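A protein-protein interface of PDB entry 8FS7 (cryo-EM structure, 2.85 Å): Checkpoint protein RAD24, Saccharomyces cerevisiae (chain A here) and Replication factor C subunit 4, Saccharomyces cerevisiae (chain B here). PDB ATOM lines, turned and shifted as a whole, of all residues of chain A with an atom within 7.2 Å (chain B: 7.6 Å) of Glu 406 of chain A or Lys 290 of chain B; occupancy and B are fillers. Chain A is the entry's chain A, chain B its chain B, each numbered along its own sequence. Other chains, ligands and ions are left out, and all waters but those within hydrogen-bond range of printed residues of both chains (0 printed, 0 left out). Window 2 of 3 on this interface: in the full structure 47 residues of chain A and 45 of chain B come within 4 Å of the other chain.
Printed residues of chain B within 4 Å of Glu 406 of chain A: Lys 290.
Of the printed residues of chain A, Lys 290 of chain B touches Glu 406 (3.5 Å) and Tyr 419 (3.5 Å).
No residue of chain B comes within 4 Å of Ser 405 of chain A.
Printed residues of chain B within 4 Å of Asn 411 of chain A: Met 297.
Of the printed residues of chain A, Ile 289 of chain B touches Glu 415 and Tyr 419.
Printed residues of chain A within 4 Å of Gly 293 of chain B: Glu 415.
Of the printed residues of chain B, Glu 418 of chain A touches Phe 271.
Printed residues of chain B within 4 Å of Glu 415 of chain A: Phe 271 (3.5 Å), Ile 289 (3.6 Å), Ile 292 (3.8 Å), Gly 293 (3.6 Å) and His 296 (3.5 Å).
Glu 287 of chain B touches none of the printed residues of chain A.
The nearest residue of chain B that does not touch Glu 406 of chain A is Leu 294 of chain B (5.8 Å).
The nearest residue of chain A that does not touch Lys 290 of chain B is Met 410 of chain A (4.2 Å).
The nearest printed residue of chain A that does not touch Met 297 of chain B is Met 410 of chain A (4.2 Å).
The side-chain sulfur of Met 297 of chain B lies close to the backbone carbonyl oxygen of Asn 409 of chain A (3.5 Å).
OE1 of Glu 406 of chain A is in salt-bridge range of NZ of Lys 290 of chain B (3.5 Å).
The side-chain amide nitrogen (ND2) of Asn 411 of chain A sits at hydrogen-bond distance from the side-chain sulfur (SD) of Met 297 of chain B, at 3.2 Å.
Among the printed residues, pairs that only touch across the chains: Tyr 419 of chain A with Leu 286 of chain B (3.3 Å), Glu 423 of chain A with Leu 286 of chain B (3.3 Å), Tyr 419 of chain A with Lys 290 of chain B (3.5 Å), Glu 415 of chain A with Phe 271 of chain B (3.5 Å), Glu 415 of chain A with His 296 of chain B (3.5 Å), Glu 415 of chain A with Gly 293 of chain B (3.6 Å), Glu 415 of chain A with Ile 289 of chain B (3.6 Å), Glu 418 of chain A with Phe 271 of chain B (3.7 Å), Glu 415 of chain A with Ile 292 of chain B (3.8 Å) and Tyr 419 of chain A with Ile 289 of chain B (3.8 Å).
Of the 19 printed residues of chain A, 7 touch a printed residue of chain B.
Hydrophobic or aromatic side chains of chain A within 4 Å of the printed part of chain B: Tyr 419.
Among the printed residues, 13 pairs touch across the chains.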
ATOM      1  N   LYS A 377     -38.114  12.853  -2.265  1.00  0.00           N
ATOM      2  CA  LYS A 377     -37.043  13.821  -2.046  1.00  0.00           C
ATOM      3  C   LYS A 377     -37.048  14.898  -3.124  1.00  0.00           C
ATOM      4  O   LYS A 377     -36.830  16.081  -2.832  1.00  0.00           O
ATOM      5  CB  LYS A 377     -35.692  13.109  -2.000  1.00  0.00           C
ATOM      6  CG  LYS A 377     -35.318  12.581  -0.624  1.00  0.00           C
ATOM      7  CD  LYS A 377     -33.859  12.860  -0.302  1.00  0.00           C
ATOM      8  CE  LYS A 377     -32.942  11.856  -0.983  1.00  0.00           C
ATOM      9  NZ  LYS A 377     -33.115  10.484  -0.432  1.00  0.00           N
ATOM     10  N   SER A 399     -29.409  25.025   4.154  1.00  0.00           N
ATOM     11  CA  SER A 399     -29.376  23.864   5.036  1.00  0.00           C
ATOM     12  C   SER A 399     -30.239  22.732   4.493  1.00  0.00           C
ATOM     13  O   SER A 399     -29.831  21.564   4.516  1.00  0.00           O
ATOM     14  CB  SER A 399     -29.831  24.259   6.441  1.00  0.00           C
ATOM     15  OG  SER A 399     -29.065  25.342   6.939  1.00  0.00           O
ATOM     16  N   ILE A 400     -31.432  23.061   3.988  1.00  0.00           N
ATOM     17  CA  ILE A 400     -32.330  22.034   3.462  1.00  0.00           C
ATOM     18  C   ILE A 400     -31.706  21.338   2.258  1.00  0.00           C
ATOM     19  O   ILE A 400     -31.693  20.102   2.167  1.00  0.00           O
ATOM     20  CB  ILE A 400     -33.699  22.645   3.114  1.00  0.00           C
ATOM     21  CG1 ILE A 400     -34.456  23.028   4.387  1.00  0.00           C
ATOM     22  CG2 ILE A 400     -34.524  21.677   2.276  1.00  0.00           C
ATOM     23  CD1 ILE A 400     -35.799  23.675   4.126  1.00  0.00           C
ATOM     24  N   VAL A 401     -31.166  22.118   1.316  1.00  0.00           N
ATOM     25  CA  VAL A 401     -30.616  21.512   0.106  1.00  0.00           C
ATOM     26  C   VAL A 401     -29.325  20.756   0.416  1.00  0.00           C
ATOM     27  O   VAL A 401     -29.038  19.723  -0.200  1.00  0.00           O
ATOM     28  CB  VAL A 401     -30.420  22.568  -0.998  1.00  0.00           C
ATOM     29  CG1 VAL A 401     -31.757  23.185  -1.380  1.00  0.00           C
ATOM     30  CG2 VAL A 401     -29.445  23.635  -0.565  1.00  0.00           C
ATOM     31  N   ASP A 402     -28.534  21.242   1.380  1.00  0.00           N
ATOM     32  CA  ASP A 402     -27.337  20.515   1.790  1.00  0.00           C
ATOM     33  C   ASP A 402     -27.698  19.184   2.435  1.00  0.00           C
ATOM     34  O   ASP A 402     -27.049  18.164   2.175  1.00  0.00           O
ATOM     35  CB  ASP A 402     -26.511  21.371   2.749  1.00  0.00           C
ATOM     36  CG  ASP A 402     -25.131  20.798   3.002  1.00  0.00           C
ATOM     37  OD1 ASP A 402     -24.703  19.914   2.232  1.00  0.00           O
ATOM     38  OD2 ASP A 402     -24.475  21.231   3.972  1.00  0.00           O
ATOM     39  N   CYS A 403     -28.737  19.173   3.275  1.00  0.00           N
ATOM     40  CA  CYS A 403     -29.192  17.924   3.870  1.00  0.00           C
ATOM     41  C   CYS A 403     -29.700  16.960   2.807  1.00  0.00           C
ATOM     42  O   CYS A 403     -29.437  15.755   2.876  1.00  0.00           O
ATOM     43  CB  CYS A 403     -30.280  18.203   4.905  1.00  0.00           C
ATOM     44  SG  CYS A 403     -31.235  16.750   5.370  1.00  0.00           S
ATOM     45  N   LEU A 404     -30.433  17.471   1.814  1.00  0.00           N
ATOM     46  CA  LEU A 404     -30.917  16.609   0.738  1.00  0.00           C
ATOM     47  C   LEU A 404     -29.763  16.031  -0.076  1.00  0.00           C
ATOM     48  O   LEU A 404     -29.785  14.851  -0.446  1.00  0.00           O
ATOM     49  CB  LEU A 404     -31.882  17.384  -0.160  1.00  0.00           C
ATOM     50  CG  LEU A 404     -33.375  17.126   0.064  1.00  0.00           C
ATOM     51  CD1 LEU A 404     -33.735  17.205   1.539  1.00  0.00           C
ATOM     52  CD2 LEU A 404     -34.212  18.106  -0.742  1.00  0.00           C
ATOM     53  N   SER A 405     -28.743  16.846  -0.358  1.00  0.00           N
ATOM     54  CA  SER A 405     -27.574  16.351  -1.078  1.00  0.00           C
ATOM     55  C   SER A 405     -26.830  15.297  -0.267  1.00  0.00           C
ATOM     56  O   SER A 405     -26.335  14.310  -0.822  1.00  0.00           O
ATOM     57  CB  SER A 405     -26.645  17.512  -1.433  1.00  0.00           C
ATOM     58  OG  SER A 405     -25.992  18.012  -0.279  1.00  0.00           O
ATOM     59  N   GLU A 406     -26.729  15.499   1.050  1.00  0.00           N
ATOM     60  CA  GLU A 406     -26.109  14.494   1.909  1.00  0.00           C
ATOM     61  C   GLU A 406     -26.910  13.196   1.909  1.00  0.00           C
ATOM     62  O   GLU A 406     -26.335  12.102   1.885  1.00  0.00           O
ATOM     63  CB  GLU A 406     -25.968  15.035   3.332  1.00  0.00           C
ATOM     64  CG  GLU A 406     -24.600  15.617   3.643  1.00  0.00           C
ATOM     65  CD  GLU A 406     -24.674  16.805   4.581  1.00  0.00           C
ATOM     66  OE1 GLU A 406     -25.761  17.056   5.141  1.00  0.00           O
ATOM     67  OE2 GLU A 406     -23.644  17.489   4.759  1.00  0.00           O
ATOM     68  N   CYS A 407     -28.242  13.302   1.942  1.00  0.00           N
ATOM     69  CA  CYS A 407     -29.090  12.115   1.918  1.00  0.00           C
ATOM     70  C   CYS A 407     -28.997  11.381   0.589  1.00  0.00           C
ATOM     71  O   CYS A 407     -29.156  10.155   0.545  1.00  0.00           O
ATOM     72  CB  CYS A 407     -30.542  12.500   2.202  1.00  0.00           C
ATOM     73  SG  CYS A 407     -30.835  13.132   3.863  1.00  0.00           S
ATOM     74  N   ASP A 408     -28.748  12.110  -0.502  1.00  0.00           N
ATOM     75  CA  ASP A 408     -28.626  11.481  -1.813  1.00  0.00           C
ATOM     76  C   ASP A 408     -27.419  10.552  -1.910  1.00  0.00           C
ATOM     77  O   ASP A 408     -27.364   9.724  -2.826  1.00  0.00           O
ATOM     78  CB  ASP A 408     -28.546  12.553  -2.900  1.00  0.00           C
ATOM     79  CG  ASP A 408     -28.788  11.994  -4.290  1.00  0.00           C
ATOM     80  OD1 ASP A 408     -29.844  11.363  -4.504  1.00  0.00           O
ATOM     81  OD2 ASP A 408     -27.922  12.187  -5.169  1.00  0.00           O
ATOM     82  N   ASN A 409     -26.459  10.661  -0.992  1.00  0.00           N
ATOM     83  CA  ASN A 409     -25.240   9.864  -1.029  1.00  0.00           C
ATOM     84  C   ASN A 409     -25.295   8.642  -0.121  1.00  0.00           C
ATOM     85  O   ASN A 409     -24.279   7.960   0.041  1.00  0.00           O
ATOM     86  CB  ASN A 409     -24.036  10.729  -0.652  1.00  0.00           C
ATOM     87  CG  ASN A 409     -23.690  11.743  -1.719  1.00  0.00           C
ATOM     88  OD1 ASN A 409     -24.372  11.849  -2.737  1.00  0.00           O
ATOM     89  ND2 ASN A 409     -22.621  12.494  -1.491  1.00  0.00           N
ATOM     90  N   MET A 410     -26.449   8.347   0.475  1.00  0.00           N
ATOM     91  CA  MET A 410     -26.580   7.235   1.405  1.00  0.00           C
ATOM     92  C   MET A 410     -27.153   5.982   0.754  1.00  0.00           C
ATOM     93  O   MET A 410     -27.466   5.019   1.463  1.00  0.00           O
ATOM     94  CB  MET A 410     -27.439   7.647   2.601  1.00  0.00           C
ATOM     95  CG  MET A 410     -26.711   8.523   3.610  1.00  0.00           C
ATOM     96  SD  MET A 410     -27.473   8.497   5.243  1.00  0.00           S
ATOM     97  CE  MET A 410     -27.398  10.234   5.678  1.00  0.00           C
ATOM     98  N   ASN A 411     -27.295   5.977  -0.574  1.00  0.00           N
ATOM     99  CA  ASN A 411     -27.735   4.806  -1.340  1.00  0.00           C
ATOM    100  C   ASN A 411     -29.097   4.292  -0.876  1.00  0.00           C
ATOM    101  O   ASN A 411     -29.321   3.085  -0.767  1.00  0.00           O
ATOM    102  CB  ASN A 411     -26.688   3.688  -1.291  1.00  0.00           C
ATOM    103  CG  ASN A 411     -25.268   4.216  -1.345  1.00  0.00           C
ATOM    104  OD1 ASN A 411     -24.810   4.694  -2.383  1.00  0.00           O
ATOM    105  ND2 ASN A 411     -24.562   4.131  -0.224  1.00  0.00           N
ATOM    106  N   GLU A 415     -32.246   5.535   7.017  1.00  0.00           N
ATOM    107  CA  GLU A 415     -31.703   6.640   7.798  1.00  0.00           C
ATOM    108  C   GLU A 415     -31.620   7.918   6.978  1.00  0.00           C
ATOM    109  O   GLU A 415     -31.821   9.010   7.518  1.00  0.00           O
ATOM    110  CB  GLU A 415     -30.322   6.275   8.338  1.00  0.00           C
ATOM    111  CG  GLU A 415     -30.333   5.265   9.470  1.00  0.00           C
ATOM    112  CD  GLU A 415     -29.877   3.889   9.030  1.00  0.00           C
ATOM    113  OE1 GLU A 415     -30.279   3.451   7.932  1.00  0.00           O
ATOM    114  OE2 GLU A 415     -29.117   3.245   9.784  1.00  0.00           O
ATOM    115  N   SER A 416     -31.332   7.804   5.680  1.00  0.00           N
ATOM    116  CA  SER A 416     -31.274   8.986   4.825  1.00  0.00           C
ATOM    117  C   SER A 416     -32.630   9.680   4.752  1.00  0.00           C
ATOM    118  O   SER A 416     -32.726  10.898   4.935  1.00  0.00           O
ATOM    119  CB  SER A 416     -30.796   8.598   3.426  1.00  0.00           C
ATOM    120  OG  SER A 416     -31.815   7.928   2.707  1.00  0.00           O
ATOM    121  N   GLU A 418     -35.167   9.364   6.852  1.00  0.00           N
ATOM    122  CA  GLU A 418     -35.519   9.863   8.179  1.00  0.00           C
ATOM    123  C   GLU A 418     -34.809  11.177   8.478  1.00  0.00           C
ATOM    124  O   GLU A 418     -35.438  12.148   8.915  1.00  0.00           O
ATOM    125  CB  GLU A 418     -35.178   8.817   9.242  1.00  0.00           C
ATOM    126  CG  GLU A 418     -35.978   7.527   9.143  1.00  0.00           C
ATOM    127  CD  GLU A 418     -37.236   7.551   9.987  1.00  0.00           C
ATOM    128  OE1 GLU A 418     -37.379   8.472  10.817  1.00  0.00           O
ATOM    129  OE2 GLU A 418     -38.076   6.643   9.826  1.00  0.00           O
ATOM    130  N   TYR A 419     -33.496  11.229   8.233  1.00  0.00           N
ATOM    131  CA  TYR A 419     -32.727  12.439   8.505  1.00  0.00           C
ATOM    132  C   TYR A 419     -33.187  13.597   7.630  1.00  0.00           C
ATOM    133  O   TYR A 419     -33.317  14.728   8.112  1.00  0.00           O
ATOM    134  CB  TYR A 419     -31.236  12.162   8.301  1.00  0.00           C
ATOM    135  CG  TYR A 419     -30.373  13.400   8.183  1.00  0.00           C
ATOM    136  CD1 TYR A 419     -30.342  14.352   9.196  1.00  0.00           C
ATOM    137  CD2 TYR A 419     -29.583  13.613   7.062  1.00  0.00           C
ATOM    138  CE1 TYR A 419     -29.553  15.481   9.088  1.00  0.00           C
ATOM    139  CE2 TYR A 419     -28.792  14.739   6.947  1.00  0.00           C
ATOM    140  CZ  TYR A 419     -28.780  15.670   7.963  1.00  0.00           C
ATOM    141  OH  TYR A 419     -27.993  16.792   7.852  1.00  0.00           O
ATOM    142  N   GLU A 423     -34.830  16.919   9.234  1.00  0.00           N
ATOM    143  CA  GLU A 423     -34.167  18.207   9.064  1.00  0.00           C
ATOM    144  C   GLU A 423     -35.081  19.217   8.383  1.00  0.00           C
ATOM    145  O   GLU A 423     -35.130  20.384   8.789  1.00  0.00           O
ATOM    146  CB  GLU A 423     -32.873  18.031   8.271  1.00  0.00           C
ATOM    147  CG  GLU A 423     -32.270  19.334   7.765  1.00  0.00           C
ATOM    148  CD  GLU A 423     -31.393  20.013   8.797  1.00  0.00           C
ATOM    149  OE1 GLU A 423     -30.697  19.301   9.550  1.00  0.00           O
ATOM    150  OE2 GLU A 423     -31.399  21.261   8.855  1.00  0.00           O
ATOM    151  N   PHE B 271     -30.284   2.682  15.418  1.00  0.00           N
ATOM    152  CA  PHE B 271     -31.233   3.422  14.591  1.00  0.00           C
ATOM    153  C   PHE B 271     -32.647   3.314  15.151  1.00  0.00           C
ATOM    154  O   PHE B 271     -33.366   4.316  15.252  1.00  0.00           O
ATOM    155  CB  PHE B 271     -31.179   2.913  13.150  1.00  0.00           C
ATOM    156  CG  PHE B 271     -32.194   3.549  12.240  1.00  0.00           C
ATOM    157  CD1 PHE B 271     -32.413   4.917  12.267  1.00  0.00           C
ATOM    158  CD2 PHE B 271     -32.926   2.775  11.354  1.00  0.00           C
ATOM    159  CE1 PHE B 271     -33.345   5.500  11.430  1.00  0.00           C
ATOM    160  CE2 PHE B 271     -33.858   3.354  10.514  1.00  0.00           C
ATOM    161  CZ  PHE B 271     -34.067   4.717  10.551  1.00  0.00           C
ATOM    162  N   THR B 274     -32.875   5.348  18.445  1.00  0.00           N
ATOM    163  CA  THR B 274     -32.928   6.778  18.156  1.00  0.00           C
ATOM    164  C   THR B 274     -34.281   7.173  17.578  1.00  0.00           C
ATOM    165  O   THR B 274     -34.796   8.260  17.868  1.00  0.00           O
ATOM    166  CB  THR B 274     -31.798   7.157  17.198  1.00  0.00           C
ATOM    167  OG1 THR B 274     -30.544   6.735  17.749  1.00  0.00           O
ATOM    168  CG2 THR B 274     -31.761   8.660  16.984  1.00  0.00           C
ATOM    169  N   VAL B 284     -30.820  17.267  17.702  1.00  0.00           N
ATOM    170  CA  VAL B 284     -29.908  16.238  18.188  1.00  0.00           C
ATOM    171  C   VAL B 284     -30.310  14.872  17.644  1.00  0.00           C
ATOM    172  O   VAL B 284     -29.459  14.085  17.210  1.00  0.00           O
ATOM    173  CB  VAL B 284     -29.869  16.254  19.728  1.00  0.00           C
ATOM    174  CG1 VAL B 284     -29.333  14.940  20.273  1.00  0.00           C
ATOM    175  CG2 VAL B 284     -29.034  17.425  20.224  1.00  0.00           C
ATOM    176  N   ARG B 285     -31.614  14.578  17.644  1.00  0.00           N
ATOM    177  CA  ARG B 285     -32.088  13.289  17.154  1.00  0.00           C
ATOM    178  C   ARG B 285     -31.759  13.098  15.678  1.00  0.00           C
ATOM    179  O   ARG B 285     -31.286  12.028  15.276  1.00  0.00           O
ATOM    180  CB  ARG B 285     -33.593  13.162  17.383  1.00  0.00           C
ATOM    181  CG  ARG B 285     -34.162  11.802  17.018  1.00  0.00           C
ATOM    182  CD  ARG B 285     -35.671  11.862  16.864  1.00  0.00           C
ATOM    183  NE  ARG B 285     -36.291  12.715  17.869  1.00  0.00           N
ATOM    184  CZ  ARG B 285     -36.638  12.309  19.082  1.00  0.00           C
ATOM    185  NH1 ARG B 285     -36.433  11.063  19.479  1.00  0.00           N
ATOM    186  NH2 ARG B 285     -37.202  13.175  19.920  1.00  0.00           N
ATOM    187  N   LEU B 286     -31.983  14.126  14.855  1.00  0.00           N
ATOM    188  CA  LEU B 286     -31.692  13.984  13.431  1.00  0.00           C
ATOM    189  C   LEU B 286     -30.193  13.926  13.162  1.00  0.00           C
ATOM    190  O   LEU B 286     -29.762  13.220  12.243  1.00  0.00           O
ATOM    191  CB  LEU B 286     -32.350  15.110  12.628  1.00  0.00           C
ATOM    192  CG  LEU B 286     -32.010  16.579  12.882  1.00  0.00           C
ATOM    193  CD1 LEU B 286     -30.883  17.063  11.985  1.00  0.00           C
ATOM    194  CD2 LEU B 286     -33.252  17.432  12.677  1.00  0.00           C
ATOM    195  N   GLU B 287     -29.380  14.644  13.945  1.00  0.00           N
ATOM    196  CA  GLU B 287     -27.934  14.531  13.781  1.00  0.00           C
ATOM    197  C   GLU B 287     -27.442  13.131  14.134  1.00  0.00           C
ATOM    198  O   GLU B 287     -26.594  12.568  13.427  1.00  0.00           O
ATOM    199  CB  GLU B 287     -27.221  15.587  14.625  1.00  0.00           C
ATOM    200  CG  GLU B 287     -27.356  17.002  14.085  1.00  0.00           C
ATOM    201  CD  GLU B 287     -26.770  17.156  12.694  1.00  0.00           C
ATOM    202  OE1 GLU B 287     -25.739  16.514  12.404  1.00  0.00           O
ATOM    203  OE2 GLU B 287     -27.344  17.919  11.888  1.00  0.00           O
ATOM    204  N   MET B 288     -27.966  12.545  15.214  1.00  0.00           N
ATOM    205  CA  MET B 288     -27.586  11.175  15.552  1.00  0.00           C
ATOM    206  C   MET B 288     -28.099  10.186  14.513  1.00  0.00           C
ATOM    207  O   MET B 288     -27.434   9.187  14.222  1.00  0.00           O
ATOM    208  CB  MET B 288     -28.079  10.805  16.953  1.00  0.00           C
ATOM    209  CG  MET B 288     -27.581  11.736  18.047  1.00  0.00           C
ATOM    210  SD  MET B 288     -28.219  11.398  19.702  1.00  0.00           S
ATOM    211  CE  MET B 288     -29.463  10.157  19.368  1.00  0.00           C
ATOM    212  N   ILE B 289     -29.272  10.451  13.932  1.00  0.00           N
ATOM    213  CA  ILE B 289     -29.773   9.603  12.851  1.00  0.00           C
ATOM    214  C   ILE B 289     -28.836   9.659  11.649  1.00  0.00           C
ATOM    215  O   ILE B 289     -28.521   8.629  11.042  1.00  0.00           O
ATOM    216  CB  ILE B 289     -31.211  10.007  12.472  1.00  0.00           C
ATOM    217  CG1 ILE B 289     -32.205   9.475  13.504  1.00  0.00           C
ATOM    218  CG2 ILE B 289     -31.572   9.508  11.079  1.00  0.00           C
ATOM    219  CD1 ILE B 289     -33.654   9.712  13.144  1.00  0.00           C
ATOM    220  N   LYS B 290     -28.374  10.860  11.294  1.00  0.00           N
ATOM    221  CA  LYS B 290     -27.440  10.999  10.179  1.00  0.00           C
ATOM    222  C   LYS B 290     -26.124  10.281  10.461  1.00  0.00           C
ATOM    223  O   LYS B 290     -25.569   9.612   9.578  1.00  0.00           O
ATOM    224  CB  LYS B 290     -27.189  12.479   9.889  1.00  0.00           C
ATOM    225  CG  LYS B 290     -26.113  12.737   8.847  1.00  0.00           C
ATOM    226  CD  LYS B 290     -25.716  14.203   8.815  1.00  0.00           C
ATOM    227  CE  LYS B 290     -24.528  14.434   7.897  1.00  0.00           C
ATOM    228  NZ  LYS B 290     -24.054  15.844   7.947  1.00  0.00           N
ATOM    229  N   GLU B 291     -25.607  10.411  11.686  1.00  0.00           N
ATOM    230  CA  GLU B 291     -24.363   9.730  12.036  1.00  0.00           C
ATOM    231  C   GLU B 291     -24.529   8.214  11.999  1.00  0.00           C
ATOM    232  O   GLU B 291     -23.647   7.498  11.506  1.00  0.00           O
ATOM    233  CB  GLU B 291     -23.888  10.187  13.414  1.00  0.00           C
ATOM    234  CG  GLU B 291     -22.452  10.674  13.433  1.00  0.00           C
ATOM    235  CD  GLU B 291     -22.287  12.025  12.764  1.00  0.00           C
ATOM    236  OE1 GLU B 291     -21.646  12.085  11.692  1.00  0.00           O
ATOM    237  OE2 GLU B 291     -22.797  13.026  13.308  1.00  0.00           O
ATOM    238  N   ILE B 292     -25.657   7.711  12.505  1.00  0.00           N
ATOM    239  CA  ILE B 292     -25.925   6.277  12.471  1.00  0.00           C
ATOM    240  C   ILE B 292     -26.064   5.797  11.032  1.00  0.00           C
ATOM    241  O   ILE B 292     -25.624   4.698  10.687  1.00  0.00           O
ATOM    242  CB  ILE B 292     -27.174   5.950  13.314  1.00  0.00           C
ATOM    243  CG1 ILE B 292     -26.862   6.108  14.804  1.00  0.00           C
ATOM    244  CG2 ILE B 292     -27.681   4.543  13.034  1.00  0.00           C
ATOM    245  CD1 ILE B 292     -28.064   5.931  15.700  1.00  0.00           C
ATOM    246  N   GLY B 293     -26.659   6.620  10.165  1.00  0.00           N
ATOM    247  CA  GLY B 293     -26.762   6.251   8.762  1.00  0.00           C
ATOM    248  C   GLY B 293     -25.416   6.191   8.064  1.00  0.00           C
ATOM    249  O   GLY B 293     -25.163   5.287   7.261  1.00  0.00           O
ATOM    250  N   LEU B 294     -24.538   7.155   8.350  1.00  0.00           N
ATOM    251  CA  LEU B 294     -23.191   7.114   7.787  1.00  0.00           C
ATOM    252  C   LEU B 294     -22.430   5.887   8.275  1.00  0.00           C
ATOM    253  O   LEU B 294     -21.744   5.213   7.492  1.00  0.00           O
ATOM    254  CB  LEU B 294     -22.433   8.394   8.139  1.00  0.00           C
ATOM    255  CG  LEU B 294     -22.967   9.692   7.531  1.00  0.00           C
ATOM    256  CD1 LEU B 294     -22.074  10.866   7.902  1.00  0.00           C
ATOM    257  CD2 LEU B 294     -23.094   9.568   6.020  1.00  0.00           C
ATOM    258  N   THR B 295     -22.548   5.575   9.568  1.00  0.00           N
ATOM    259  CA  THR B 295     -21.914   4.373  10.099  1.00  0.00           C
ATOM    260  C   THR B 295     -22.499   3.116   9.464  1.00  0.00           C
ATOM    261  O   THR B 295     -21.770   2.163   9.176  1.00  0.00           O
ATOM    262  CB  THR B 295     -22.060   4.336  11.621  1.00  0.00           C
ATOM    263  OG1 THR B 295     -21.420   5.487  12.183  1.00  0.00           O
ATOM    264  CG2 THR B 295     -21.417   3.083  12.197  1.00  0.00           C
ATOM    265  N   HIS B 296     -23.813   3.103   9.231  1.00  0.00           N
ATOM    266  CA  HIS B 296     -24.457   1.969   8.573  1.00  0.00           C
ATOM    267  C   HIS B 296     -23.929   1.782   7.160  1.00  0.00           C
ATOM    268  O   HIS B 296     -23.693   0.651   6.722  1.00  0.00           O
ATOM    269  CB  HIS B 296     -25.972   2.179   8.551  1.00  0.00           C
ATOM    270  CG  HIS B 296     -26.745   0.975   8.114  1.00  0.00           C
ATOM    271  ND1 HIS B 296     -27.467   0.940   6.941  1.00  0.00           N
ATOM    272  CD2 HIS B 296     -26.920  -0.234   8.698  1.00  0.00           C
ATOM    273  CE1 HIS B 296     -28.047  -0.241   6.818  1.00  0.00           C
ATOM    274  NE2 HIS B 296     -27.730  -0.971   7.871  1.00  0.00           N
ATOM    275  N   MET B 297     -23.748   2.884   6.429  1.00  0.00           N
ATOM    276  CA  MET B 297     -23.171   2.802   5.091  1.00  0.00           C
ATOM    277  C   MET B 297     -21.751   2.253   5.138  1.00  0.00           C
ATOM    278  O   MET B 297     -21.371   1.416   4.310  1.00  0.00           O
ATOM    279  CB  MET B 297     -23.193   4.179   4.429  1.00  0.00           C
ATOM    280  CG  MET B 297     -23.511   4.151   2.945  1.00  0.00           C
ATOM    281  SD  MET B 297     -22.796   5.542   2.048  1.00  0.00           S
ATOM    282  CE  MET B 297     -22.880   6.833   3.287  1.00  0.00           C
ATOM    283  N   MET B 312     -18.569   6.421  15.763  1.00  0.00           N
ATOM    284  CA  MET B 312     -19.972   6.820  15.805  1.00  0.00           C
ATOM    285  C   MET B 312     -20.359   7.325  17.188  1.00  0.00           C
ATOM    286  O   MET B 312     -21.027   8.359  17.316  1.00  0.00           O
ATOM    287  CB  MET B 312     -20.864   5.649  15.396  1.00  0.00           C
ATOM    288  CG  MET B 312     -22.329   6.017  15.217  1.00  0.00           C
ATOM    289  SD  MET B 312     -23.433   4.607  15.429  1.00  0.00           S
ATOM    290  CE  MET B 312     -23.047   4.122  17.108  1.00  0.00           C
ATOM    291  N   LEU B 319     -21.786  15.803  19.201  1.00  0.00           N
ATOM    292  CA  LEU B 319     -22.994  16.552  18.872  1.00  0.00           C
ATOM    293  C   LEU B 319     -23.877  16.749  20.099  1.00  0.00           C
ATOM    294  O   LEU B 319     -24.622  17.733  20.174  1.00  0.00           O
ATOM    295  CB  LEU B 319     -23.750  15.849  17.737  1.00  0.00           C
ATOM    296  CG  LEU B 319     -24.705  14.664  17.942  1.00  0.00           C
ATOM    297  CD1 LEU B 319     -26.115  15.084  18.370  1.00  0.00           C
ATOM    298  CD2 LEU B 319     -24.754  13.807  16.685  1.00  0.00           C
